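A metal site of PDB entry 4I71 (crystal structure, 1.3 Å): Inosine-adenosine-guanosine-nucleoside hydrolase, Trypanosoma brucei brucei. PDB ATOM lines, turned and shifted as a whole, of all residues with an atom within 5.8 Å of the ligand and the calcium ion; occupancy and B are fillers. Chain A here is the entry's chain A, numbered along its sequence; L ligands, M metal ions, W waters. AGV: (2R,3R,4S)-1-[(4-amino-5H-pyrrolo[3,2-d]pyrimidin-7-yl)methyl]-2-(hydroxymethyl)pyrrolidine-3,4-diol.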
ATOM      1  N   HIS A  12       8.516  13.280 -25.251  1.00  0.00           N
ATOM      2  CA  HIS A  12       7.080  13.439 -25.288  1.00  0.00           C
ATOM      3  C   HIS A  12       6.533  13.520 -26.679  1.00  0.00           C
ATOM      4  O   HIS A  12       7.297  13.652 -27.646  1.00  0.00           O
ATOM      5  CB  HIS A  12       6.653  14.637 -24.479  1.00  0.00           C
ATOM      6  CG  HIS A  12       6.921  15.959 -25.095  1.00  0.00           C
ATOM      7  ND1 HIS A  12       6.053  16.516 -26.012  1.00  0.00           N
ATOM      8  CD2 HIS A  12       7.926  16.844 -24.908  1.00  0.00           C
ATOM      9  CE1 HIS A  12       6.541  17.691 -26.378  1.00  0.00           C
ATOM     10  NE2 HIS A  12       7.665  17.925 -25.726  1.00  0.00           N
ATOM     11  N   ASP A  13       5.209  13.425 -26.806  1.00  0.00           N
ATOM     12  CA  ASP A  13       4.564  13.554 -28.111  1.00  0.00           C
ATOM     13  C   ASP A  13       3.463  14.570 -28.159  1.00  0.00           C
ATOM     14  O   ASP A  13       2.563  14.474 -28.990  1.00  0.00           O
ATOM     15  CB  ASP A  13       4.086  12.205 -28.598  1.00  0.00           C
ATOM     16  CG  ASP A  13       2.941  11.636 -27.825  1.00  0.00           C
ATOM     17  OD1 ASP A  13       2.761  12.029 -26.640  1.00  0.00           O
ATOM     18  OD2 ASP A  13       2.212  10.767 -28.435  1.00  0.00           O
ATOM     19  N   GLY A  14       3.545  15.595 -27.298  1.00  0.00           N
ATOM     20  CA  GLY A  14       2.874  16.865 -27.596  1.00  0.00           C
ATOM     21  C   GLY A  14       1.364  16.926 -27.494  1.00  0.00           C
ATOM     22  O   GLY A  14       0.795  17.828 -28.114  1.00  0.00           O
ATOM     23  N   ASN A  15       0.726  16.014 -26.763  1.00  0.00           N
ATOM     24  CA  ASN A  15      -0.669  16.223 -26.451  1.00  0.00           C
ATOM     25  C   ASN A  15      -0.774  17.139 -25.188  1.00  0.00           C
ATOM     26  O   ASN A  15       0.238  17.512 -24.579  1.00  0.00           O
ATOM     27  CB  ASN A  15      -1.437  14.915 -26.282  1.00  0.00           C
ATOM     28  CG  ASN A  15      -2.870  15.047 -26.851  1.00  0.00           C
ATOM     29  OD1 ASN A  15      -3.810  15.249 -26.090  1.00  0.00           O
ATOM     30  ND2 ASN A  15      -3.022  14.993 -28.152  1.00  0.00           N
ATOM     31  N   LYS A  16      -1.998  17.514 -24.830  1.00  0.00           N
ATOM     32  CA  LYS A  16      -2.185  18.413 -23.707  1.00  0.00           C
ATOM     33  C   LYS A  16      -1.528  17.891 -22.458  1.00  0.00           C
ATOM     34  O   LYS A  16      -0.838  18.632 -21.727  1.00  0.00           O
ATOM     35  CB  LYS A  16      -3.703  18.644 -23.489  1.00  0.00           C
ATOM     36  CG  LYS A  16      -4.361  19.413 -24.654  1.00  0.00           C
ATOM     37  CD  LYS A  16      -5.874  19.149 -24.759  1.00  0.00           C
ATOM     38  CE  LYS A  16      -6.104  17.709 -25.229  1.00  0.00           C
ATOM     39  NZ  LYS A  16      -7.586  17.478 -25.362  1.00  0.00           N
ATOM     40  N   ASP A  17      -1.725  16.609 -22.221  1.00  0.00           N
ATOM     41  CA  ASP A  17      -1.221  15.909 -21.085  1.00  0.00           C
ATOM     42  C   ASP A  17       0.338  15.958 -21.010  1.00  0.00           C
ATOM     43  O   ASP A  17       0.952  16.089 -19.974  1.00  0.00           O
ATOM     44  CB  ASP A  17      -1.751  14.475 -21.218  1.00  0.00           C
ATOM     45  CG  ASP A  17      -1.379  13.569 -20.099  1.00  0.00           C
ATOM     46  OD1 ASP A  17      -1.274  13.992 -18.902  1.00  0.00           O
ATOM     47  OD2 ASP A  17      -1.225  12.357 -20.438  1.00  0.00           O
ATOM     48  N   ASP A  18       0.949  15.809 -22.164  1.00  0.00           N
ATOM     49  CA  ASP A  18       2.439  15.895 -22.289  1.00  0.00           C
ATOM     50  C   ASP A  18       2.958  17.241 -21.751  1.00  0.00           C
ATOM     51  O   ASP A  18       3.992  17.306 -21.086  1.00  0.00           O
ATOM     52  CB  ASP A  18       2.904  15.699 -23.733  1.00  0.00           C
ATOM     53  CG  ASP A  18       2.589  14.326 -24.256  1.00  0.00           C
ATOM     54  OD1 ASP A  18       3.490  13.439 -24.182  1.00  0.00           O
ATOM     55  OD2 ASP A  18       1.435  14.097 -24.719  1.00  0.00           O
ATOM     56  N   ASP A  43       1.200  11.840 -31.052  1.00  0.00           N
ATOM     57  CA  ASP A  43      -0.094  12.486 -30.671  1.00  0.00           C
ATOM     58  C   ASP A  43      -0.088  13.991 -30.852  1.00  0.00           C
ATOM     59  O   ASP A  43      -0.795  14.723 -30.121  1.00  0.00           O
ATOM     60  CB  ASP A  43      -0.459  12.080 -29.238  1.00  0.00           C
ATOM     61  CG  ASP A  43      -1.930  12.055 -28.924  1.00  0.00           C
ATOM     62  OD1 ASP A  43      -2.771  12.160 -29.827  1.00  0.00           O
ATOM     63  OD2 ASP A  43      -2.233  11.898 -27.699  1.00  0.00           O
ATOM     64  N   PHE A  82      -1.821   8.055 -34.715  1.00  0.00           N
ATOM     65  CA  PHE A  82      -2.887   8.552 -33.891  1.00  0.00           C
ATOM     66  C   PHE A  82      -4.019   9.101 -34.703  1.00  0.00           C
ATOM     67  O   PHE A  82      -3.833   9.547 -35.830  1.00  0.00           O
ATOM     68  CB  PHE A  82      -2.390   9.641 -32.915  1.00  0.00           C
ATOM     69  CG  PHE A  82      -1.776   9.092 -31.640  1.00  0.00           C
ATOM     70  CD1 PHE A  82      -2.608   8.747 -30.579  1.00  0.00           C
ATOM     71  CD2 PHE A  82      -0.426   8.890 -31.509  1.00  0.00           C
ATOM     72  CE1 PHE A  82      -2.130   8.246 -29.440  1.00  0.00           C
ATOM     73  CE2 PHE A  82       0.082   8.377 -30.338  1.00  0.00           C
ATOM     74  CZ  PHE A  82      -0.760   8.051 -29.297  1.00  0.00           C
ATOM     75  N   TRP A  86      -7.085  14.101 -32.533  1.00  0.00           N
ATOM     76  CA  TRP A  86      -6.314  14.209 -31.285  1.00  0.00           C
ATOM     77  C   TRP A  86      -5.010  14.984 -31.493  1.00  0.00           C
ATOM     78  O   TRP A  86      -4.521  15.693 -30.610  1.00  0.00           O
ATOM     79  CB  TRP A  86      -5.991  12.849 -30.722  1.00  0.00           C
ATOM     80  CG  TRP A  86      -7.200  12.079 -30.209  1.00  0.00           C
ATOM     81  CD1 TRP A  86      -8.493  12.509 -30.093  1.00  0.00           C
ATOM     82  CD2 TRP A  86      -7.177  10.749 -29.728  1.00  0.00           C
ATOM     83  NE1 TRP A  86      -9.262  11.506 -29.583  1.00  0.00           N
ATOM     84  CE2 TRP A  86      -8.484  10.410 -29.350  1.00  0.00           C
ATOM     85  CE3 TRP A  86      -6.163   9.804 -29.576  1.00  0.00           C
ATOM     86  CZ2 TRP A  86      -8.805   9.145 -28.829  1.00  0.00           C
ATOM     87  CZ3 TRP A  86      -6.488   8.546 -29.062  1.00  0.00           C
ATOM     88  CH2 TRP A  86      -7.788   8.240 -28.714  1.00  0.00           C
ATOM     89  N   THR A 140       6.711   9.988 -22.357  1.00  0.00           N
ATOM     90  CA  THR A 140       5.280  10.201 -22.327  1.00  0.00           C
ATOM     91  C   THR A 140       4.635  10.057 -23.696  1.00  0.00           C
ATOM     92  O   THR A 140       3.427  10.229 -23.858  1.00  0.00           O
ATOM     93  CB  THR A 140       4.933  11.530 -21.687  1.00  0.00           C
ATOM     94  OG1 THR A 140       5.525  12.594 -22.467  1.00  0.00           O
ATOM     95  CG2 THR A 140       5.440  11.599 -20.274  1.00  0.00           C
ATOM     96  N   GLY A 141       5.410   9.724 -24.713  1.00  0.00           N
ATOM     97  CA  GLY A 141       4.923   9.289 -25.991  1.00  0.00           C
ATOM     98  C   GLY A 141       5.381   7.862 -26.272  1.00  0.00           C
ATOM     99  O   GLY A 141       5.774   7.134 -25.348  1.00  0.00           O
ATOM    100  N   MET A 167       4.976   6.297 -19.617  1.00  0.00           N
ATOM    101  CA  MET A 167       3.507   6.196 -19.734  1.00  0.00           C
ATOM    102  C   MET A 167       3.230   5.264 -20.897  1.00  0.00           C
ATOM    103  O   MET A 167       3.545   5.576 -22.032  1.00  0.00           O
ATOM    104  CB  MET A 167       2.893   7.566 -19.899  1.00  0.00           C
ATOM    105  CG  MET A 167       1.407   7.544 -19.650  1.00  0.00           C
ATOM    106  SD  MET A 167       0.450   6.770 -21.002  1.00  0.00           S
ATOM    107  CE  MET A 167      -0.547   5.491 -20.130  1.00  0.00           C
ATOM    108  N   ASN A 176      -7.060   1.316 -24.494  1.00  0.00           N
ATOM    109  CA  ASN A 176      -7.756   2.505 -24.952  1.00  0.00           C
ATOM    110  C   ASN A 176      -7.735   2.679 -26.466  1.00  0.00           C
ATOM    111  O   ASN A 176      -8.162   3.746 -26.950  1.00  0.00           O
ATOM    112  CB  ASN A 176      -7.308   3.752 -24.171  1.00  0.00           C
ATOM    113  CG  ASN A 176      -5.885   4.158 -24.391  1.00  0.00           C
ATOM    114  OD1 ASN A 176      -5.219   3.627 -25.308  1.00  0.00           O
ATOM    115  ND2 ASN A 176      -5.411   5.138 -23.591  1.00  0.00           N
ATOM    116  N   GLU A 187      -2.974  -0.137 -25.394  1.00  0.00           N
ATOM    117  CA  GLU A 187      -2.870   1.293 -25.080  1.00  0.00           C
ATOM    118  C   GLU A 187      -2.112   1.995 -26.210  1.00  0.00           C
ATOM    119  O   GLU A 187      -1.259   1.411 -26.839  1.00  0.00           O
ATOM    120  CB  GLU A 187      -2.235   1.452 -23.690  1.00  0.00           C
ATOM    121  CG  GLU A 187      -1.997   2.864 -23.222  1.00  0.00           C
ATOM    122  CD  GLU A 187      -0.820   3.552 -23.907  1.00  0.00           C
ATOM    123  OE1 GLU A 187       0.182   2.853 -24.231  1.00  0.00           O
ATOM    124  OE2 GLU A 187      -0.879   4.821 -24.126  1.00  0.00           O
ATOM    125  N   TRP A 188      -2.487   3.246 -26.474  1.00  0.00           N
ATOM    126  CA  TRP A 188      -2.079   3.964 -27.673  1.00  0.00           C
ATOM    127  C   TRP A 188      -0.558   4.155 -27.831  1.00  0.00           C
ATOM    128  O   TRP A 188      -0.025   4.008 -28.940  1.00  0.00           O
ATOM    129  CB  TRP A 188      -2.807   5.340 -27.757  1.00  0.00           C
ATOM    130  CG  TRP A 188      -4.039   5.264 -28.585  1.00  0.00           C
ATOM    131  CD1 TRP A 188      -5.346   5.217 -28.185  1.00  0.00           C
ATOM    132  CD2 TRP A 188      -4.044   5.210 -30.011  1.00  0.00           C
ATOM    133  NE1 TRP A 188      -6.152   5.139 -29.276  1.00  0.00           N
ATOM    134  CE2 TRP A 188      -5.389   5.118 -30.413  1.00  0.00           C
ATOM    135  CE3 TRP A 188      -3.042   5.200 -30.976  1.00  0.00           C
ATOM    136  CZ2 TRP A 188      -5.750   5.033 -31.753  1.00  0.00           C
ATOM    137  CZ3 TRP A 188      -3.398   5.135 -32.329  1.00  0.00           C
ATOM    138  CH2 TRP A 188      -4.739   5.047 -32.684  1.00  0.00           C
ATOM    139  N   ASN A 189       0.147   4.535 -26.774  1.00  0.00           N
ATOM    140  CA  ASN A 189       1.574   4.784 -26.897  1.00  0.00           C
ATOM    141  C   ASN A 189       2.323   3.537 -27.366  1.00  0.00           C
ATOM    142  O   ASN A 189       3.271   3.617 -28.149  1.00  0.00           O
ATOM    143  CB  ASN A 189       2.211   5.299 -25.605  1.00  0.00           C
ATOM    144  CG  ASN A 189       1.846   6.720 -25.303  1.00  0.00           C
ATOM    145  OD1 ASN A 189       1.287   7.431 -26.155  1.00  0.00           O
ATOM    146  ND2 ASN A 189       2.145   7.146 -24.071  1.00  0.00           N
ATOM    147  N   LEU A 213      -2.315   1.903 -17.893  1.00  0.00           N
ATOM    148  CA  LEU A 213      -3.683   2.350 -17.628  1.00  0.00           C
ATOM    149  C   LEU A 213      -4.158   1.855 -16.241  1.00  0.00           C
ATOM    150  O   LEU A 213      -5.030   2.474 -15.627  1.00  0.00           O
ATOM    151  CB  LEU A 213      -4.640   1.959 -18.743  1.00  0.00           C
ATOM    152  CG  LEU A 213      -4.331   2.486 -20.159  1.00  0.00           C
ATOM    153  CD1 LEU A 213      -5.442   2.091 -21.119  1.00  0.00           C
ATOM    154  CD2 LEU A 213      -4.074   3.977 -20.125  1.00  0.00           C
ATOM    155  N   GLU A 251     -14.635  14.732 -22.337  1.00  0.00           N
ATOM    156  CA  GLU A 251     -14.410  13.463 -23.032  1.00  0.00           C
ATOM    157  C   GLU A 251     -15.004  12.291 -22.269  1.00  0.00           C
ATOM    158  O   GLU A 251     -15.460  11.332 -22.861  1.00  0.00           O
ATOM    159  CB  GLU A 251     -12.928  13.228 -23.312  1.00  0.00           C
ATOM    160  CG  GLU A 251     -12.395  14.300 -24.295  1.00  0.00           C
ATOM    161  CD  GLU A 251     -11.029  14.039 -24.874  1.00  0.00           C
ATOM    162  OE1 GLU A 251     -10.603  12.855 -24.906  1.00  0.00           O
ATOM    163  OE2 GLU A 251     -10.371  15.041 -25.295  1.00  0.00           O
ATOM    164  N   ARG A 255     -17.495   9.871 -24.297  1.00  0.00           N
ATOM    165  CA  ARG A 255     -17.139   8.466 -24.455  1.00  0.00           C
ATOM    166  C   ARG A 255     -17.619   7.582 -23.293  1.00  0.00           C
ATOM    167  O   ARG A 255     -17.053   6.537 -23.030  1.00  0.00           O
ATOM    168  CB  ARG A 255     -15.644   8.318 -24.698  1.00  0.00           C
ATOM    169  CG  ARG A 255     -15.182   8.910 -25.994  1.00  0.00           C
ATOM    170  CD  ARG A 255     -13.735   8.328 -26.394  1.00  0.00           C
ATOM    171  NE  ARG A 255     -12.787   8.742 -25.358  1.00  0.00           N
ATOM    172  CZ  ARG A 255     -12.142   9.906 -25.331  1.00  0.00           C
ATOM    173  NH1 ARG A 255     -12.274  10.795 -26.294  1.00  0.00           N
ATOM    174  NH2 ARG A 255     -11.359  10.166 -24.271  1.00  0.00           N
ATOM    175  N   ALA A 259     -12.510   8.436 -20.219  1.00  0.00           N
ATOM    176  CA  ALA A 259     -12.109   9.817 -20.007  1.00  0.00           C
ATOM    177  C   ALA A 259     -10.808  10.212 -20.738  1.00  0.00           C
ATOM    178  O   ALA A 259     -10.068   9.375 -21.228  1.00  0.00           O
ATOM    179  CB  ALA A 259     -11.936  10.068 -18.503  1.00  0.00           C
ATOM    180  N   TYR A 260     -10.577  11.501 -20.758  1.00  0.00           N
ATOM    181  CA  TYR A 260      -9.195  11.997 -20.895  1.00  0.00           C
ATOM    182  C   TYR A 260      -8.638  11.938 -19.487  1.00  0.00           C
ATOM    183  O   TYR A 260      -9.261  12.408 -18.533  1.00  0.00           O
ATOM    184  CB  TYR A 260      -9.211  13.411 -21.508  1.00  0.00           C
ATOM    185  CG  TYR A 260      -7.850  13.892 -22.000  1.00  0.00           C
ATOM    186  CD1 TYR A 260      -7.529  13.821 -23.361  1.00  0.00           C
ATOM    187  CD2 TYR A 260      -6.914  14.401 -21.151  1.00  0.00           C
ATOM    188  CE1 TYR A 260      -6.291  14.260 -23.844  1.00  0.00           C
ATOM    189  CE2 TYR A 260      -5.645  14.855 -21.621  1.00  0.00           C
ATOM    190  CZ  TYR A 260      -5.352  14.762 -22.988  1.00  0.00           C
ATOM    191  OH  TYR A 260      -4.106  15.212 -23.420  1.00  0.00           O
ATOM    192  N   TRP A 263      -2.639  11.060 -17.726  1.00  0.00           N
ATOM    193  CA  TRP A 263      -1.742   9.928 -17.945  1.00  0.00           C
ATOM    194  C   TRP A 263      -0.278  10.325 -17.755  1.00  0.00           C
ATOM    195  O   TRP A 263       0.457   9.749 -16.908  1.00  0.00           O
ATOM    196  CB  TRP A 263      -1.926   9.361 -19.291  1.00  0.00           C
ATOM    197  CG  TRP A 263      -3.202   8.871 -19.830  1.00  0.00           C
ATOM    198  CD1 TRP A 263      -3.744   7.641 -19.675  1.00  0.00           C
ATOM    199  CD2 TRP A 263      -4.105   9.571 -20.735  1.00  0.00           C
ATOM    200  NE1 TRP A 263      -4.914   7.521 -20.413  1.00  0.00           N
ATOM    201  CE2 TRP A 263      -5.158   8.684 -21.066  1.00  0.00           C
ATOM    202  CE3 TRP A 263      -4.120  10.877 -21.260  1.00  0.00           C
ATOM    203  CZ2 TRP A 263      -6.186   9.032 -21.926  1.00  0.00           C
ATOM    204  CZ3 TRP A 263      -5.142  11.217 -22.130  1.00  0.00           C
ATOM    205  CH2 TRP A 263      -6.160  10.311 -22.440  1.00  0.00           C
ATOM    206  N   ASP A 264       0.173  11.267 -18.551  1.00  0.00           N
ATOM    207  CA  ASP A 264       1.552  11.687 -18.550  1.00  0.00           C
ATOM    208  C   ASP A 264       1.891  12.536 -17.353  1.00  0.00           C
ATOM    209  O   ASP A 264       3.033  12.499 -16.833  1.00  0.00           O
ATOM    210  CB  ASP A 264       1.839  12.492 -19.841  1.00  0.00           C
ATOM    211  CG  ASP A 264       1.647  11.709 -21.128  1.00  0.00           C
ATOM    212  OD1 ASP A 264       1.516  10.468 -21.038  1.00  0.00           O
ATOM    213  OD2 ASP A 264       1.582  12.379 -22.181  1.00  0.00           O
HETATM  214  O5' AGV L   1      -2.813   6.589 -24.240  1.00  0.00           O
HETATM  215  C5' AGV L   1      -2.451   7.749 -23.484  1.00  0.00           C
HETATM  216  C4' AGV L   1      -1.388   8.639 -24.117  1.00  0.00           C
HETATM  217  C3' AGV L   1      -0.763   9.637 -23.135  1.00  0.00           C
HETATM  218  O3' AGV L   1       0.658   9.721 -23.301  1.00  0.00           O
HETATM  219  N4' AGV L   1      -1.888   9.540 -25.218  1.00  0.00           N
HETATM  220  C1' AGV L   1      -2.416  10.766 -24.525  1.00  0.00           C
HETATM  221  C2' AGV L   1      -1.460  10.979 -23.422  1.00  0.00           C
HETATM  222  O2' AGV L   1      -0.542  12.025 -23.817  1.00  0.00           O
HETATM  223  C7  AGV L   1      -2.766   8.929 -26.341  1.00  0.00           C
HETATM  224  C9  AGV L   1      -4.233   9.145 -26.134  1.00  0.00           C
HETATM  225  C8  AGV L   1      -5.095   8.190 -25.647  1.00  0.00           C
HETATM  226  N7  AGV L   1      -6.337   8.723 -25.591  1.00  0.00           N
HETATM  227  C5  AGV L   1      -6.324  10.027 -26.027  1.00  0.00           C
HETATM  228  C4  AGV L   1      -5.003  10.298 -26.376  1.00  0.00           C
HETATM  229  C6  AGV L   1      -7.313  11.011 -26.138  1.00  0.00           C
HETATM  230  N6  AGV L   1      -8.587  10.826 -25.773  1.00  0.00           N
HETATM  231  N1  AGV L   1      -6.929  12.220 -26.627  1.00  0.00           N
HETATM  232  C2  AGV L   1      -5.661  12.399 -26.963  1.00  0.00           C
HETATM  233  N3  AGV L   1      -4.671  11.500 -26.874  1.00  0.00           N
HETATM  234 CA    CA M   1       1.739  11.648 -24.566  1.00  0.00          CA
HETATM  235  O   HOH W   1       0.714  10.053 -26.244  1.00  0.00           O
HETATM  236  O   HOH W   2      -8.253  14.727 -26.731  1.00  0.00           O
HETATM  237  O   HOH W   3      -8.907   7.885 -24.990  1.00  0.00           O
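The guanidinium group (NH2) of Arg 255 lies close to a nitrogen (N6) of the ligand (3.2 Å). OD1 of Asn 15 touches C2 of the ligand, at 3.5 Å. Phe 82 touches the ligand. Trp 86 touches the ligand (CZ3 to C5, 3.4 Å). Trp 188 touches the ligand (CB to O5', 3.7 Å). Tyr 260 touches the ligand. CE3 of Trp 263 touches C2' of the ligand, at 3.4 Å. Hydrophobic or aromatic side chains that line the ligand: Phe 82, Trp 86, Met 167, Trp 188, Tyr 260 and Trp 263.
Water W1 bridges OD1 of Asn 189 (2.7 Å) and OD2 of Asp 13 (2.7 Å). Water W3 bridges a nitrogen (N7) of the ligand and the guanidinium group of Arg 255. Water W2 lies within hydrogen-bond range of the side-chain carboxylate of Glu 251 (2.6 Å), a nitrogen (N1) of the ligand (2.8 Å) and the side-chain amino group of Lys 16 (3.1 Å).
Four residues have an atom within 4 Å of the calcium ion: Asp 13, Asp 18, Thr 140 and Asp 264. Along chain A the residues within 4 Å of the calcium ion span positions 13 to 264.
O of Thr 140 is bound to the calcium ion (2.3 Å). The calcium ion is bound by OD1 of Asp 13, 2.3 Å away. The calcium ion is bound by O2' of the ligand (2.4 Å). The side-chain carboxylate (OD2) of Asp 18 is bound to the calcium ion (2.5 Å). OD2 of Asp 264 is bound to the calcium ion, at 2.5 Å. The calcium ion is bound by water W1, at 2.5 Å. OD1 of Asp 18 is bound to the calcium ion, at 2.5 Å. O3' of the ligand is bound to the calcium ion, at 2.5 Å. The calcium ion has eight donor atoms within binding distance.
The side-chain carboxylate (OD2) of Asp 43 lies within salt-bridge range of a nitrogen (N4') of the ligand (3.4 Å). OE2 of Glu 187 sits at hydrogen-bond distance from O5' of the ligand, 2.6 Å away. N6 of the ligand sits at hydrogen-bond distance from OE1 of Glu 251 (3.0 Å). The side-chain amide nitrogen (ND2) of Asn 176 sits at hydrogen-bond distance from an oxygen (O5') of the ligand (3.0 Å). An oxygen (O3') of the ligand sits close to the side-chain amide nitrogen (ND2) of Asn 189 (3.1 Å). An oxygen (O2') of the ligand lies close to the side-chain carboxylate (OD2) of Asp 17, 3.5 Å away. The side-chain sulfur of Met 167 lies close to an oxygen (O3') of the ligand.
The side-chain carboxylate of Asp 13 sits at hydrogen-bond distance from the backbone NH of Asp 43. OD2 of Asp 18 lies close to N of Asn 15, 2.9 Å away. N of Asp 264 sits at hydrogen-bond distance from OD2 of Asp 17. The side-chain carboxylate (OE2) of Glu 187 sits at hydrogen-bond distance from the backbone NH (N) of Asn 189, at 2.9 Å. The side-chain amide nitrogen (ND2) of Asn 189 sits at hydrogen-bond distance from the backbone carbonyl oxygen (O) of Met 167, 2.9 Å away. OD2 of Asp 17 lies close to N of Trp 263 (3.3 Å). The side-chain hydroxyl of Tyr 260 sits at hydrogen-bond distance from the backbone NH of Asp 17 (3.0 Å). OH of Tyr 260 is in hydrogen-bond range of N of Lys 16, 3.4 Å away.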
